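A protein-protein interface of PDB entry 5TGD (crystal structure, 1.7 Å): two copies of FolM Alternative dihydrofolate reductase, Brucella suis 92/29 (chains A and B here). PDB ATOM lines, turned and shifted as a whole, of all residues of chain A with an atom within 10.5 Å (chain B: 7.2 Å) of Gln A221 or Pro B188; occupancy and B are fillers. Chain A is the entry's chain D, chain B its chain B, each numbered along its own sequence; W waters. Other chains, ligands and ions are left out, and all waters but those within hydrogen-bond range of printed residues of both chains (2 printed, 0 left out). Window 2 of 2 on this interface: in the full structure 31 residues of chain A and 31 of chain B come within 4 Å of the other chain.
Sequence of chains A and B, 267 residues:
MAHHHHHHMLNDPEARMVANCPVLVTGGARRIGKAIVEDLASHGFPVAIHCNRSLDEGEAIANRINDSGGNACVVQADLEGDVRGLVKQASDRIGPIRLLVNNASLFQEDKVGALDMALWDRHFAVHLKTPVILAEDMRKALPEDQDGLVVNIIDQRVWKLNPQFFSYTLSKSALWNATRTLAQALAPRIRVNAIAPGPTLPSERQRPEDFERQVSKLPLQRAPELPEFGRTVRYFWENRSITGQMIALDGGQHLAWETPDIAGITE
O of Gly B148 sits at hydrogen-bond distance from N of Arg B191, at 2.9 Å. The side-chain amide nitrogen (NE2) of Gln A221 lies within hydrogen-bond range of the backbone carbonyl oxygen (O) of Ser A216 (3.1 Å). N of Leu A220 lies within hydrogen-bond range of O of Gly A251 (3.0 Å). The side-chain carboxylate (OE1) of Glu A225 is in salt-bridge range of the guanidinium group (NH2) of Arg A222, 3.4 Å away. The side-chain carboxylate (OE2) of Glu A228 lies within hydrogen-bond range of the backbone NH (N) of Glu A225, 2.9 Å away.
Printed residues of chain B within 4 Å of Gln A221: Pro B188. Of the printed residues of chain A, Pro B188 touches Pro A219, Leu A220 and Gln A221. Of chain A, only Pro A219 (3.3 Å) and Leu A220 (3.9 Å) come within 4 Å of Ala B187. Printed residues of chain A within 4 Å of Gln B184: Leu A255 and Trp A257. Of the printed residues of chain B, Glu A228 touches Arg B240 (3.4 Å). Of the printed residues of chain B, Arg A222 touches Arg B240. Arg B139 touches none of the printed residues of chain A. Glu A225 touches none of the printed residues of chain B. The nearest printed residue of chain B that does not touch Gln A221 is Ala B187 (6.1 Å). The nearest printed residue of chain A that does not touch Pro B188 is Leu A218 (5.9 Å).
Pro A219 touches Ala B187. Pro B188 touches Pro A219 (CB to O, 3.4 Å). CD2 of Leu A220 touches CB of Ala B187, 3.9 Å away. O of Leu A220 touches CB of Pro B188, at 3.7 Å. Leu A220 touches Arg B191 (CD1 to CD, 3.96 Å). O of Arg B240 touches CD1 of Leu A220 (3.5 Å). OE1 of Gln A221 touches CG of Pro B188, at 3.3 Å. Arg B240 touches Arg A222. Trp A257 touches Gln B184 (CD1 to NE2, 3.7 Å).
The side-chain amide nitrogen (NE2) of Gln B184 lies within hydrogen-bond range of the backbone carbonyl oxygen (O) of Leu A255 (3.0 Å). N of Arg B240 sits at hydrogen-bond distance from OE1 of Glu A228, 3.4 Å away.
Hydrophobic or aromatic side chains of chain A that line the printed part of chain B: Leu A220 and Trp A257. Along chain A the printed residues that touch a printed residue of chain B span positions 219 to 257.
Water W1 bridges O of Gln B184 (2.6 Å) and NE1 of Trp A257 (3.1 Å). Water W2 bridges the backbone carbonyl oxygen of Leu A220 (3.0 Å) and the backbone carbonyl oxygen of Pro B188 (3.4 Å).
No position is printed for both chains. Of the 11 pairs that touch across the chains among the printed residues, none has its exchanged pair printed and touching as well.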
ATOM      1  N   PRO A 199      35.846  11.662  11.084  1.00  0.00           N
ATOM      2  CA  PRO A 199      36.480  12.928  11.486  1.00  0.00           C
ATOM      3  C   PRO A 199      35.781  13.559  12.680  1.00  0.00           C
ATOM      4  O   PRO A 199      34.686  14.115  12.562  1.00  0.00           O
ATOM      5  CB  PRO A 199      36.357  13.798  10.227  1.00  0.00           C
ATOM      6  CG  PRO A 199      35.137  13.275   9.522  1.00  0.00           C
ATOM      7  CD  PRO A 199      35.092  11.788   9.818  1.00  0.00           C
ATOM      8  N   PHE A 211      38.664  20.735   7.751  1.00  0.00           N
ATOM      9  CA  PHE A 211      37.751  19.907   8.531  1.00  0.00           C
ATOM     10  C   PHE A 211      36.296  20.297   8.270  1.00  0.00           C
ATOM     11  O   PHE A 211      35.470  19.447   7.931  1.00  0.00           O
ATOM     12  CB  PHE A 211      38.075  20.018  10.029  1.00  0.00           C
ATOM     13  CG  PHE A 211      37.161  19.209  10.921  1.00  0.00           C
ATOM     14  CD1 PHE A 211      37.482  17.906  11.270  1.00  0.00           C
ATOM     15  CD2 PHE A 211      35.989  19.759  11.420  1.00  0.00           C
ATOM     16  CE1 PHE A 211      36.648  17.166  12.088  1.00  0.00           C
ATOM     17  CE2 PHE A 211      35.151  19.024  12.235  1.00  0.00           C
ATOM     18  CZ  PHE A 211      35.482  17.727  12.570  1.00  0.00           C
ATOM     19  N   GLU A 212      35.992  21.586   8.429  1.00  0.00           N
ATOM     20  CA  GLU A 212      34.604  22.033   8.343  1.00  0.00           C
ATOM     21  C   GLU A 212      33.992  21.710   6.984  1.00  0.00           C
ATOM     22  O   GLU A 212      32.818  21.326   6.899  1.00  0.00           O
ATOM     23  CB  GLU A 212      34.523  23.533   8.630  1.00  0.00           C
ATOM     24  N   ARG A 213      34.769  21.858   5.908  1.00  0.00           N
ATOM     25  CA  ARG A 213      34.236  21.588   4.576  1.00  0.00           C
ATOM     26  C   ARG A 213      34.108  20.090   4.333  1.00  0.00           C
ATOM     27  O   ARG A 213      33.161  19.641   3.675  1.00  0.00           O
ATOM     28  CB  ARG A 213      35.120  22.238   3.511  1.00  0.00           C
ATOM     29  N   GLN A 214      35.052  19.308   4.865  1.00  0.00           N
ATOM     30  CA  GLN A 214      35.003  17.857   4.732  1.00  0.00           C
ATOM     31  C   GLN A 214      33.707  17.292   5.299  1.00  0.00           C
ATOM     32  O   GLN A 214      33.085  16.407   4.697  1.00  0.00           O
ATOM     33  CB  GLN A 214      36.211  17.237   5.436  1.00  0.00           C
ATOM     34  CG  GLN A 214      36.134  15.727   5.635  1.00  0.00           C
ATOM     35  CD  GLN A 214      37.346  15.164   6.371  1.00  0.00           C
ATOM     36  OE1 GLN A 214      38.035  15.881   7.102  1.00  0.00           O
ATOM     37  NE2 GLN A 214      37.610  13.873   6.182  1.00  0.00           N
ATOM     38  N   VAL A 215      33.280  17.804   6.453  1.00  0.00           N
ATOM     39  CA  VAL A 215      32.102  17.266   7.127  1.00  0.00           C
ATOM     40  C   VAL A 215      30.856  17.449   6.267  1.00  0.00           C
ATOM     41  O   VAL A 215      30.011  16.549   6.176  1.00  0.00           O
ATOM     42  CB  VAL A 215      31.955  17.919   8.512  1.00  0.00           C
ATOM     43  CG1 VAL A 215      30.546  17.758   9.046  1.00  0.00           C
ATOM     44  CG2 VAL A 215      32.975  17.320   9.468  1.00  0.00           C
ATOM     45  N   SER A 216      30.730  18.605   5.604  1.00  0.00           N
ATOM     46  CA  SER A 216      29.586  18.835   4.726  1.00  0.00           C
ATOM     47  C   SER A 216      29.501  17.801   3.611  1.00  0.00           C
ATOM     48  O   SER A 216      28.419  17.586   3.050  1.00  0.00           O
ATOM     49  CB  SER A 216      29.656  20.238   4.126  1.00  0.00           C
ATOM     50  OG  SER A 216      30.760  20.352   3.242  1.00  0.00           O
ATOM     51  N   LYS A 217      30.614  17.151   3.283  1.00  0.00           N
ATOM     52  CA  LYS A 217      30.630  16.145   2.238  1.00  0.00           C
ATOM     53  C   LYS A 217      30.367  14.735   2.761  1.00  0.00           C
ATOM     54  O   LYS A 217      30.237  13.806   1.954  1.00  0.00           O
ATOM     55  CB  LYS A 217      31.965  16.223   1.490  1.00  0.00           C
ATOM     56  CG  LYS A 217      32.078  17.517   0.682  1.00  0.00           C
ATOM     57  CD  LYS A 217      33.495  17.833   0.225  1.00  0.00           C
ATOM     58  CE  LYS A 217      33.498  19.092  -0.650  1.00  0.00           C
ATOM     59  NZ  LYS A 217      34.861  19.518  -1.089  1.00  0.00           N
ATOM     60  N   LEU A 218      30.260  14.555   4.076  1.00  0.00           N
ATOM     61  CA  LEU A 218      29.828  13.272   4.608  1.00  0.00           C
ATOM     62  C   LEU A 218      28.353  13.045   4.285  1.00  0.00           C
ATOM     63  O   LEU A 218      27.584  14.002   4.162  1.00  0.00           O
ATOM     64  CB  LEU A 218      30.033  13.212   6.116  1.00  0.00           C
ATOM     65  CG  LEU A 218      31.456  13.393   6.634  1.00  0.00           C
ATOM     66  CD1 LEU A 218      31.440  13.528   8.158  1.00  0.00           C
ATOM     67  CD2 LEU A 218      32.326  12.245   6.190  1.00  0.00           C
ATOM     68  N   PRO A 219      27.935  11.787   4.131  1.00  0.00           N
ATOM     69  CA  PRO A 219      26.513  11.530   3.844  1.00  0.00           C
ATOM     70  C   PRO A 219      25.554  12.144   4.859  1.00  0.00           C
ATOM     71  O   PRO A 219      24.505  12.673   4.472  1.00  0.00           O
ATOM     72  CB  PRO A 219      26.455   9.997   3.821  1.00  0.00           C
ATOM     73  CG  PRO A 219      27.836   9.595   3.280  1.00  0.00           C
ATOM     74  CD  PRO A 219      28.763  10.572   3.978  1.00  0.00           C
ATOM     75  N   LEU A 220      25.890  12.108   6.145  1.00  0.00           N
ATOM     76  CA  LEU A 220      25.060  12.751   7.151  1.00  0.00           C
ATOM     77  C   LEU A 220      25.389  14.227   7.333  1.00  0.00           C
ATOM     78  O   LEU A 220      24.691  14.908   8.090  1.00  0.00           O
ATOM     79  CB  LEU A 220      25.194  12.016   8.491  1.00  0.00           C
ATOM     80  CG  LEU A 220      24.760  10.549   8.445  1.00  0.00           C
ATOM     81  CD1 LEU A 220      24.860   9.906   9.825  1.00  0.00           C
ATOM     82  CD2 LEU A 220      23.351  10.392   7.861  1.00  0.00           C
ATOM     83  N   GLN A 221      26.437  14.724   6.668  1.00  0.00           N
ATOM     84  CA  GLN A 221      26.820  16.136   6.727  1.00  0.00           C
ATOM     85  C   GLN A 221      26.984  16.618   8.168  1.00  0.00           C
ATOM     86  O   GLN A 221      26.687  17.766   8.495  1.00  0.00           O
ATOM     87  CB  GLN A 221      25.816  17.009   5.967  1.00  0.00           C
ATOM     88  CG  GLN A 221      25.510  16.485   4.572  1.00  0.00           C
ATOM     89  CD  GLN A 221      24.706  17.454   3.731  1.00  0.00           C
ATOM     90  OE1 GLN A 221      23.483  17.515   3.832  1.00  0.00           O
ATOM     91  NE2 GLN A 221      25.393  18.213   2.887  1.00  0.00           N
ATOM     92  N   ARG A 222      27.464  15.738   9.042  1.00  0.00           N
ATOM     93  CA  ARG A 222      27.717  16.101  10.427  1.00  0.00           C
ATOM     94  C   ARG A 222      28.790  15.178  10.972  1.00  0.00           C
ATOM     95  O   ARG A 222      28.875  14.006  10.593  1.00  0.00           O
ATOM     96  CB  ARG A 222      26.465  16.021  11.306  1.00  0.00           C
ATOM     97  CG  ARG A 222      25.979  14.612  11.588  1.00  0.00           C
ATOM     98  CD  ARG A 222      24.730  14.634  12.453  1.00  0.00           C
ATOM     99  NE  ARG A 222      25.018  14.992  13.842  1.00  0.00           N
ATOM    100  CZ  ARG A 222      24.796  16.190  14.381  1.00  0.00           C
ATOM    101  NH1 ARG A 222      24.279  17.169  13.649  1.00  0.00           N
ATOM    102  NH2 ARG A 222      25.087  16.410  15.660  1.00  0.00           N
ATOM    103  N   ALA A 223      29.613  15.721  11.845  1.00  0.00           N
ATOM    104  CA  ALA A 223      30.667  14.915  12.431  1.00  0.00           C
ATOM    105  C   ALA A 223      30.157  14.192  13.668  1.00  0.00           C
ATOM    106  O   ALA A 223      29.254  14.683  14.358  1.00  0.00           O
ATOM    107  CB  ALA A 223      31.857  15.791  12.812  1.00  0.00           C
ATOM    108  N   PRO A 224      30.714  13.026  13.966  1.00  0.00           N
ATOM    109  CA  PRO A 224      30.482  12.426  15.281  1.00  0.00           C
ATOM    110  C   PRO A 224      30.846  13.424  16.363  1.00  0.00           C
ATOM    111  O   PRO A 224      31.791  14.198  16.221  1.00  0.00           O
ATOM    112  CB  PRO A 224      31.425  11.222  15.292  1.00  0.00           C
ATOM    113  CG  PRO A 224      32.480  11.580  14.282  1.00  0.00           C
ATOM    114  CD  PRO A 224      31.719  12.276  13.197  1.00  0.00           C
ATOM    115  N   GLU A 225      30.087  13.411  17.447  1.00  0.00           N
ATOM    116  CA  GLU A 225      30.367  14.275  18.580  1.00  0.00           C
ATOM    117  C   GLU A 225      30.936  13.457  19.732  1.00  0.00           C
ATOM    118  O   GLU A 225      30.666  12.261  19.862  1.00  0.00           O
ATOM    119  CB  GLU A 225      29.108  15.026  19.009  1.00  0.00           C
ATOM    120  CG  GLU A 225      28.762  16.121  18.030  1.00  0.00           C
ATOM    121  CD  GLU A 225      27.418  16.731  18.293  1.00  0.00           C
ATOM    122  OE1 GLU A 225      26.521  15.997  18.755  1.00  0.00           O
ATOM    123  OE2 GLU A 225      27.263  17.944  18.037  1.00  0.00           O
ATOM    124  N   GLU A 228      29.198  10.748  21.909  1.00  0.00           N
ATOM    125  CA  GLU A 228      28.785   9.480  21.313  1.00  0.00           C
ATOM    126  C   GLU A 228      29.756   8.354  21.635  1.00  0.00           C
ATOM    127  O   GLU A 228      29.358   7.185  21.646  1.00  0.00           O
ATOM    128  CB  GLU A 228      28.641   9.612  19.794  1.00  0.00           C
ATOM    129  CG  GLU A 228      27.597  10.643  19.346  1.00  0.00           C
ATOM    130  CD  GLU A 228      27.427  10.694  17.825  1.00  0.00           C
ATOM    131  OE1 GLU A 228      27.055   9.660  17.218  1.00  0.00           O
ATOM    132  OE2 GLU A 228      27.671  11.774  17.242  1.00  0.00           O
ATOM    133  N   ASP A 250      30.844   7.902  12.320  1.00  0.00           N
ATOM    134  CA  ASP A 250      31.581   8.516  11.226  1.00  0.00           C
ATOM    135  C   ASP A 250      30.720   9.381  10.315  1.00  0.00           C
ATOM    136  O   ASP A 250      31.191   9.774   9.243  1.00  0.00           O
ATOM    137  CB  ASP A 250      32.292   7.422  10.416  1.00  0.00           C
ATOM    138  CG  ASP A 250      31.328   6.567   9.595  1.00  0.00           C
ATOM    139  OD1 ASP A 250      31.808   5.816   8.703  1.00  0.00           O
ATOM    140  OD2 ASP A 250      30.099   6.661   9.826  1.00  0.00           O
ATOM    141  N   GLY A 251      29.486   9.693  10.693  1.00  0.00           N
ATOM    142  CA  GLY A 251      28.642  10.465   9.804  1.00  0.00           C
ATOM    143  C   GLY A 251      28.392   9.811   8.466  1.00  0.00           C
ATOM    144  O   GLY A 251      28.053  10.501   7.502  1.00  0.00           O
ATOM    145  N   GLY A 252      28.548   8.494   8.384  1.00  0.00           N
ATOM    146  CA  GLY A 252      28.343   7.781   7.136  1.00  0.00           C
ATOM    147  C   GLY A 252      29.541   7.736   6.215  1.00  0.00           C
ATOM    148  O   GLY A 252      29.419   7.218   5.094  1.00  0.00           O
ATOM    149  N   GLN A 253      30.702   8.235   6.660  1.00  0.00           N
ATOM    150  CA  GLN A 253      31.868   8.341   5.785  1.00  0.00           C
ATOM    151  C   GLN A 253      32.183   7.030   5.079  1.00  0.00           C
ATOM    152  O   GLN A 253      32.500   7.027   3.884  1.00  0.00           O
ATOM    153  CB  GLN A 253      33.088   8.803   6.575  1.00  0.00           C
ATOM    154  CG  GLN A 253      34.283   9.027   5.684  1.00  0.00           C
ATOM    155  CD  GLN A 253      35.380   9.822   6.350  1.00  0.00           C
ATOM    156  OE1 GLN A 253      35.618   9.695   7.552  1.00  0.00           O
ATOM    157  NE2 GLN A 253      36.049  10.664   5.573  1.00  0.00           N
ATOM    158  N   LEU A 255      30.319   4.871   4.006  1.00  0.00           N
ATOM    159  CA  LEU A 255      29.303   4.612   2.999  1.00  0.00           C
ATOM    160  C   LEU A 255      29.374   5.581   1.829  1.00  0.00           C
ATOM    161  O   LEU A 255      28.515   5.516   0.941  1.00  0.00           O
ATOM    162  CB  LEU A 255      27.906   4.695   3.627  1.00  0.00           C
ATOM    163  CG  LEU A 255      27.607   3.733   4.769  1.00  0.00           C
ATOM    164  CD1 LEU A 255      26.251   4.043   5.344  1.00  0.00           C
ATOM    165  CD2 LEU A 255      27.657   2.300   4.282  1.00  0.00           C
ATOM    166  N   ALA A 256      30.342   6.499   1.828  1.00  0.00           N
ATOM    167  CA  ALA A 256      30.504   7.402   0.696  1.00  0.00           C
ATOM    168  C   ALA A 256      30.730   6.588  -0.569  1.00  0.00           C
ATOM    169  O   ALA A 256      31.416   5.564  -0.553  1.00  0.00           O
ATOM    170  CB  ALA A 256      31.670   8.363   0.923  1.00  0.00           C
ATOM    171  N   TRP A 257      30.155   7.056  -1.669  1.00  0.00           N
ATOM    172  CA  TRP A 257      30.075   6.220  -2.854  1.00  0.00           C
ATOM    173  C   TRP A 257      30.274   6.946  -4.174  1.00  0.00           C
ATOM    174  O   TRP A 257      30.487   6.267  -5.180  1.00  0.00           O
ATOM    175  CB  TRP A 257      28.714   5.521  -2.884  1.00  0.00           C
ATOM    176  CG  TRP A 257      27.583   6.496  -2.818  1.00  0.00           C
ATOM    177  CD1 TRP A 257      26.957   6.964  -1.695  1.00  0.00           C
ATOM    178  CD2 TRP A 257      26.960   7.147  -3.925  1.00  0.00           C
ATOM    179  NE1 TRP A 257      25.966   7.855  -2.043  1.00  0.00           N
ATOM    180  CE2 TRP A 257      25.954   7.986  -3.406  1.00  0.00           C
ATOM    181  CE3 TRP A 257      27.153   7.097  -5.310  1.00  0.00           C
ATOM    182  CZ2 TRP A 257      25.141   8.762  -4.221  1.00  0.00           C
ATOM    183  CZ3 TRP A 257      26.343   7.869  -6.122  1.00  0.00           C
ATOM    184  CH2 TRP A 257      25.347   8.690  -5.575  1.00  0.00           C
ATOM    185  N   GLU A 258      30.213   8.279  -4.220  1.00  0.00           N
ATOM    186  CA  GLU A 258      30.290   9.014  -5.488  1.00  0.00           C
ATOM    187  C   GLU A 258      31.756   9.142  -5.895  1.00  0.00           C
ATOM    188  O   GLU A 258      32.420  10.159  -5.673  1.00  0.00           O
ATOM    189  CB  GLU A 258      29.635  10.383  -5.371  1.00  0.00           C
ATOM    190  CG  GLU A 258      28.291  10.397  -4.656  1.00  0.00           C
ATOM    191  CD  GLU A 258      27.905  11.790  -4.165  1.00  0.00           C
ATOM    192  OE1 GLU A 258      28.003  12.748  -4.969  1.00  0.00           O
ATOM    193  OE2 GLU A 258      27.520  11.921  -2.977  1.00  0.00           O
ATOM    194  N   ARG B 139       9.556   9.113   5.041  1.00  0.00           N
ATOM    195  CA  ARG B 139      10.311  10.254   4.535  1.00  0.00           C
ATOM    196  C   ARG B 139       9.390  11.282   3.897  1.00  0.00           C
ATOM    197  O   ARG B 139       9.610  12.489   4.036  1.00  0.00           O
ATOM    198  CB  ARG B 139      11.370   9.801   3.528  1.00  0.00           C
ATOM    199  CG  ARG B 139      12.496  10.815   3.321  1.00  0.00           C
ATOM    200  CD  ARG B 139      12.341  11.597   2.039  1.00  0.00           C
ATOM    201  NE  ARG B 139      12.744  10.821   0.869  1.00  0.00           N
ATOM    202  CZ  ARG B 139      13.961  10.855   0.329  1.00  0.00           C
ATOM    203  NH1 ARG B 139      14.906  11.628   0.853  1.00  0.00           N
ATOM    204  NH2 ARG B 139      14.234  10.117  -0.742  1.00  0.00           N
ATOM    205  N   ASP B 147      14.685  15.228  11.785  1.00  0.00           N
ATOM    206  CA  ASP B 147      15.392  14.066  11.274  1.00  0.00           C
ATOM    207  C   ASP B 147      14.675  12.798  11.727  1.00  0.00           C
ATOM    208  O   ASP B 147      13.823  12.818  12.615  1.00  0.00           O
ATOM    209  CB  ASP B 147      16.842  14.061  11.743  1.00  0.00           C
ATOM    210  CG  ASP B 147      16.963  13.914  13.244  1.00  0.00           C
ATOM    211  OD1 ASP B 147      16.320  14.701  13.977  1.00  0.00           O
ATOM    212  OD2 ASP B 147      17.692  13.005  13.693  1.00  0.00           O
ATOM    213  N   GLY B 148      15.025  11.677  11.102  1.00  0.00           N
ATOM    214  CA  GLY B 148      14.353  10.430  11.386  1.00  0.00           C
ATOM    215  C   GLY B 148      15.318   9.262  11.390  1.00  0.00           C
ATOM    216  O   GLY B 148      16.491   9.390  11.031  1.00  0.00           O
ATOM    217  N   ALA B 183      20.173   3.825   3.506  1.00  0.00           N
ATOM    218  CA  ALA B 183      20.925   4.797   4.295  1.00  0.00           C
ATOM    219  C   ALA B 183      21.594   5.812   3.388  1.00  0.00           C
ATOM    220  O   ALA B 183      21.559   7.017   3.658  1.00  0.00           O
ATOM    221  CB  ALA B 183      21.957   4.094   5.172  1.00  0.00           C
ATOM    222  N   GLN B 184      22.177   5.343   2.284  1.00  0.00           N
ATOM    223  CA  GLN B 184      22.777   6.256   1.321  1.00  0.00           C
ATOM    224  C   GLN B 184      21.727   7.133   0.650  1.00  0.00           C
ATOM    225  O   GLN B 184      21.974   8.321   0.409  1.00  0.00           O
ATOM    226  CB  GLN B 184      23.555   5.469   0.274  1.00  0.00           C
ATOM    227  CG  GLN B 184      24.747   4.708   0.839  1.00  0.00           C
ATOM    228  CD  GLN B 184      25.279   3.698  -0.159  1.00  0.00           C
ATOM    229  OE1 GLN B 184      24.503   3.033  -0.850  1.00  0.00           O
ATOM    230  NE2 GLN B 184      26.601   3.592  -0.257  1.00  0.00           N
ATOM    231  N   ALA B 185      20.552   6.569   0.338  1.00  0.00           N
ATOM    232  CA  ALA B 185      19.531   7.336  -0.376  1.00  0.00           C
ATOM    233  C   ALA B 185      18.850   8.362   0.530  1.00  0.00           C
ATOM    234  O   ALA B 185      18.547   9.475   0.088  1.00  0.00           O
ATOM    235  CB  ALA B 185      18.486   6.399  -0.984  1.00  0.00           C
ATOM    236  N   LEU B 186      18.595   8.012   1.793  1.00  0.00           N
ATOM    237  CA  LEU B 186      17.802   8.873   2.659  1.00  0.00           C
ATOM    238  C   LEU B 186      18.640   9.838   3.485  1.00  0.00           C
ATOM    239  O   LEU B 186      18.070  10.685   4.182  1.00  0.00           O
ATOM    240  CB  LEU B 186      16.929   8.025   3.589  1.00  0.00           C
ATOM    241  CG  LEU B 186      15.889   7.145   2.894  1.00  0.00           C
ATOM    242  CD1 LEU B 186      14.982   6.475   3.903  1.00  0.00           C
ATOM    243  CD2 LEU B 186      15.081   7.978   1.939  1.00  0.00           C
ATOM    244  N   ALA B 187      19.965   9.725   3.438  1.00  0.00           N
ATOM    245  CA  ALA B 187      20.829  10.680   4.110  1.00  0.00           C
ATOM    246  C   ALA B 187      20.707  12.044   3.435  1.00  0.00           C
ATOM    247  O   ALA B 187      20.436  12.125   2.234  1.00  0.00           O
ATOM    248  CB  ALA B 187      22.281  10.206   4.071  1.00  0.00           C
ATOM    249  N   PRO B 188      20.897  13.141   4.188  1.00  0.00           N
ATOM    250  CA  PRO B 188      21.259  13.223   5.609  1.00  0.00           C
ATOM    251  C   PRO B 188      20.089  13.189   6.602  1.00  0.00           C
ATOM    252  O   PRO B 188      20.327  13.006   7.799  1.00  0.00           O
ATOM    253  CB  PRO B 188      21.948  14.580   5.695  1.00  0.00           C
ATOM    254  CG  PRO B 188      21.157  15.408   4.751  1.00  0.00           C
ATOM    255  CD  PRO B 188      20.840  14.484   3.582  1.00  0.00           C
ATOM    256  N   ARG B 189      18.851  13.367   6.136  1.00  0.00           N
ATOM    257  CA  ARG B 189      17.777  13.618   7.093  1.00  0.00           C
ATOM    258  C   ARG B 189      17.296  12.348   7.788  1.00  0.00           C
ATOM    259  O   ARG B 189      16.833  12.418   8.933  1.00  0.00           O
ATOM    260  CB  ARG B 189      16.599  14.334   6.416  1.00  0.00           C
ATOM    261  CG  ARG B 189      15.627  14.975   7.420  1.00  0.00           C
ATOM    262  CD  ARG B 189      14.672  15.998   6.782  1.00  0.00           C
ATOM    263  NE  ARG B 189      13.818  15.411   5.752  1.00  0.00           N
ATOM    264  CZ  ARG B 189      12.634  14.847   5.980  1.00  0.00           C
ATOM    265  NH1 ARG B 189      12.157  14.789   7.216  1.00  0.00           N
ATOM    266  NH2 ARG B 189      11.929  14.335   4.973  1.00  0.00           N
ATOM    267  N   ILE B 190      17.397  11.187   7.144  1.00  0.00           N
ATOM    268  CA  ILE B 190      16.915   9.946   7.734  1.00  0.00           C
ATOM    269  C   ILE B 190      18.043   8.933   7.769  1.00  0.00           C
ATOM    270  O   ILE B 190      18.689   8.667   6.746  1.00  0.00           O
ATOM    271  CB  ILE B 190      15.700   9.389   6.978  1.00  0.00           C
ATOM    272  CG1 ILE B 190      14.545  10.373   7.093  1.00  0.00           C
ATOM    273  CG2 ILE B 190      15.282   8.047   7.551  1.00  0.00           C
ATOM    274  CD1 ILE B 190      13.298   9.853   6.520  1.00  0.00           C
ATOM    275  N   ARG B 191      18.264   8.357   8.941  1.00  0.00           N
ATOM    276  CA  ARG B 191      19.243   7.299   9.116  1.00  0.00           C
ATOM    277  C   ARG B 191      18.552   5.941   9.080  1.00  0.00           C
ATOM    278  O   ARG B 191      17.385   5.805   9.462  1.00  0.00           O
ATOM    279  CB  ARG B 191      20.012   7.492  10.430  1.00  0.00           C
ATOM    280  CG  ARG B 191      20.711   8.835  10.478  1.00  0.00           C
ATOM    281  CD  ARG B 191      21.505   9.039  11.747  1.00  0.00           C
ATOM    282  NE  ARG B 191      20.649   9.253  12.904  1.00  0.00           N
ATOM    283  CZ  ARG B 191      20.639   8.496  13.998  1.00  0.00           C
ATOM    284  NH1 ARG B 191      21.455   7.453  14.109  1.00  0.00           N
ATOM    285  NH2 ARG B 191      19.809   8.803  14.993  1.00  0.00           N
ATOM    286  N   ARG B 240      23.766  10.256  16.645  1.00  0.00           N
ATOM    287  CA  ARG B 240      23.300  10.716  15.346  1.00  0.00           C
ATOM    288  C   ARG B 240      24.304  10.485  14.229  1.00  0.00           C
ATOM    289  O   ARG B 240      23.972  10.740  13.067  1.00  0.00           O
ATOM    290  CB  ARG B 240      22.936  12.201  15.432  1.00  0.00           C
ATOM    291  CG  ARG B 240      21.808  12.506  16.427  1.00  0.00           C
ATOM    292  CD  ARG B 240      21.505  14.001  16.491  1.00  0.00           C
ATOM    293  NE  ARG B 240      21.133  14.527  15.179  1.00  0.00           N
ATOM    294  CZ  ARG B 240      21.017  15.819  14.893  1.00  0.00           C
ATOM    295  NH1 ARG B 240      21.247  16.732  15.829  1.00  0.00           N
ATOM    296  NH2 ARG B 240      20.676  16.200  13.667  1.00  0.00           N
HETATM  297  O   HOH W   1      24.367   9.268   0.189  1.00  0.00           O
HETATM  298  O   HOH W   2      22.355  14.685  10.014  1.00  0.00           O
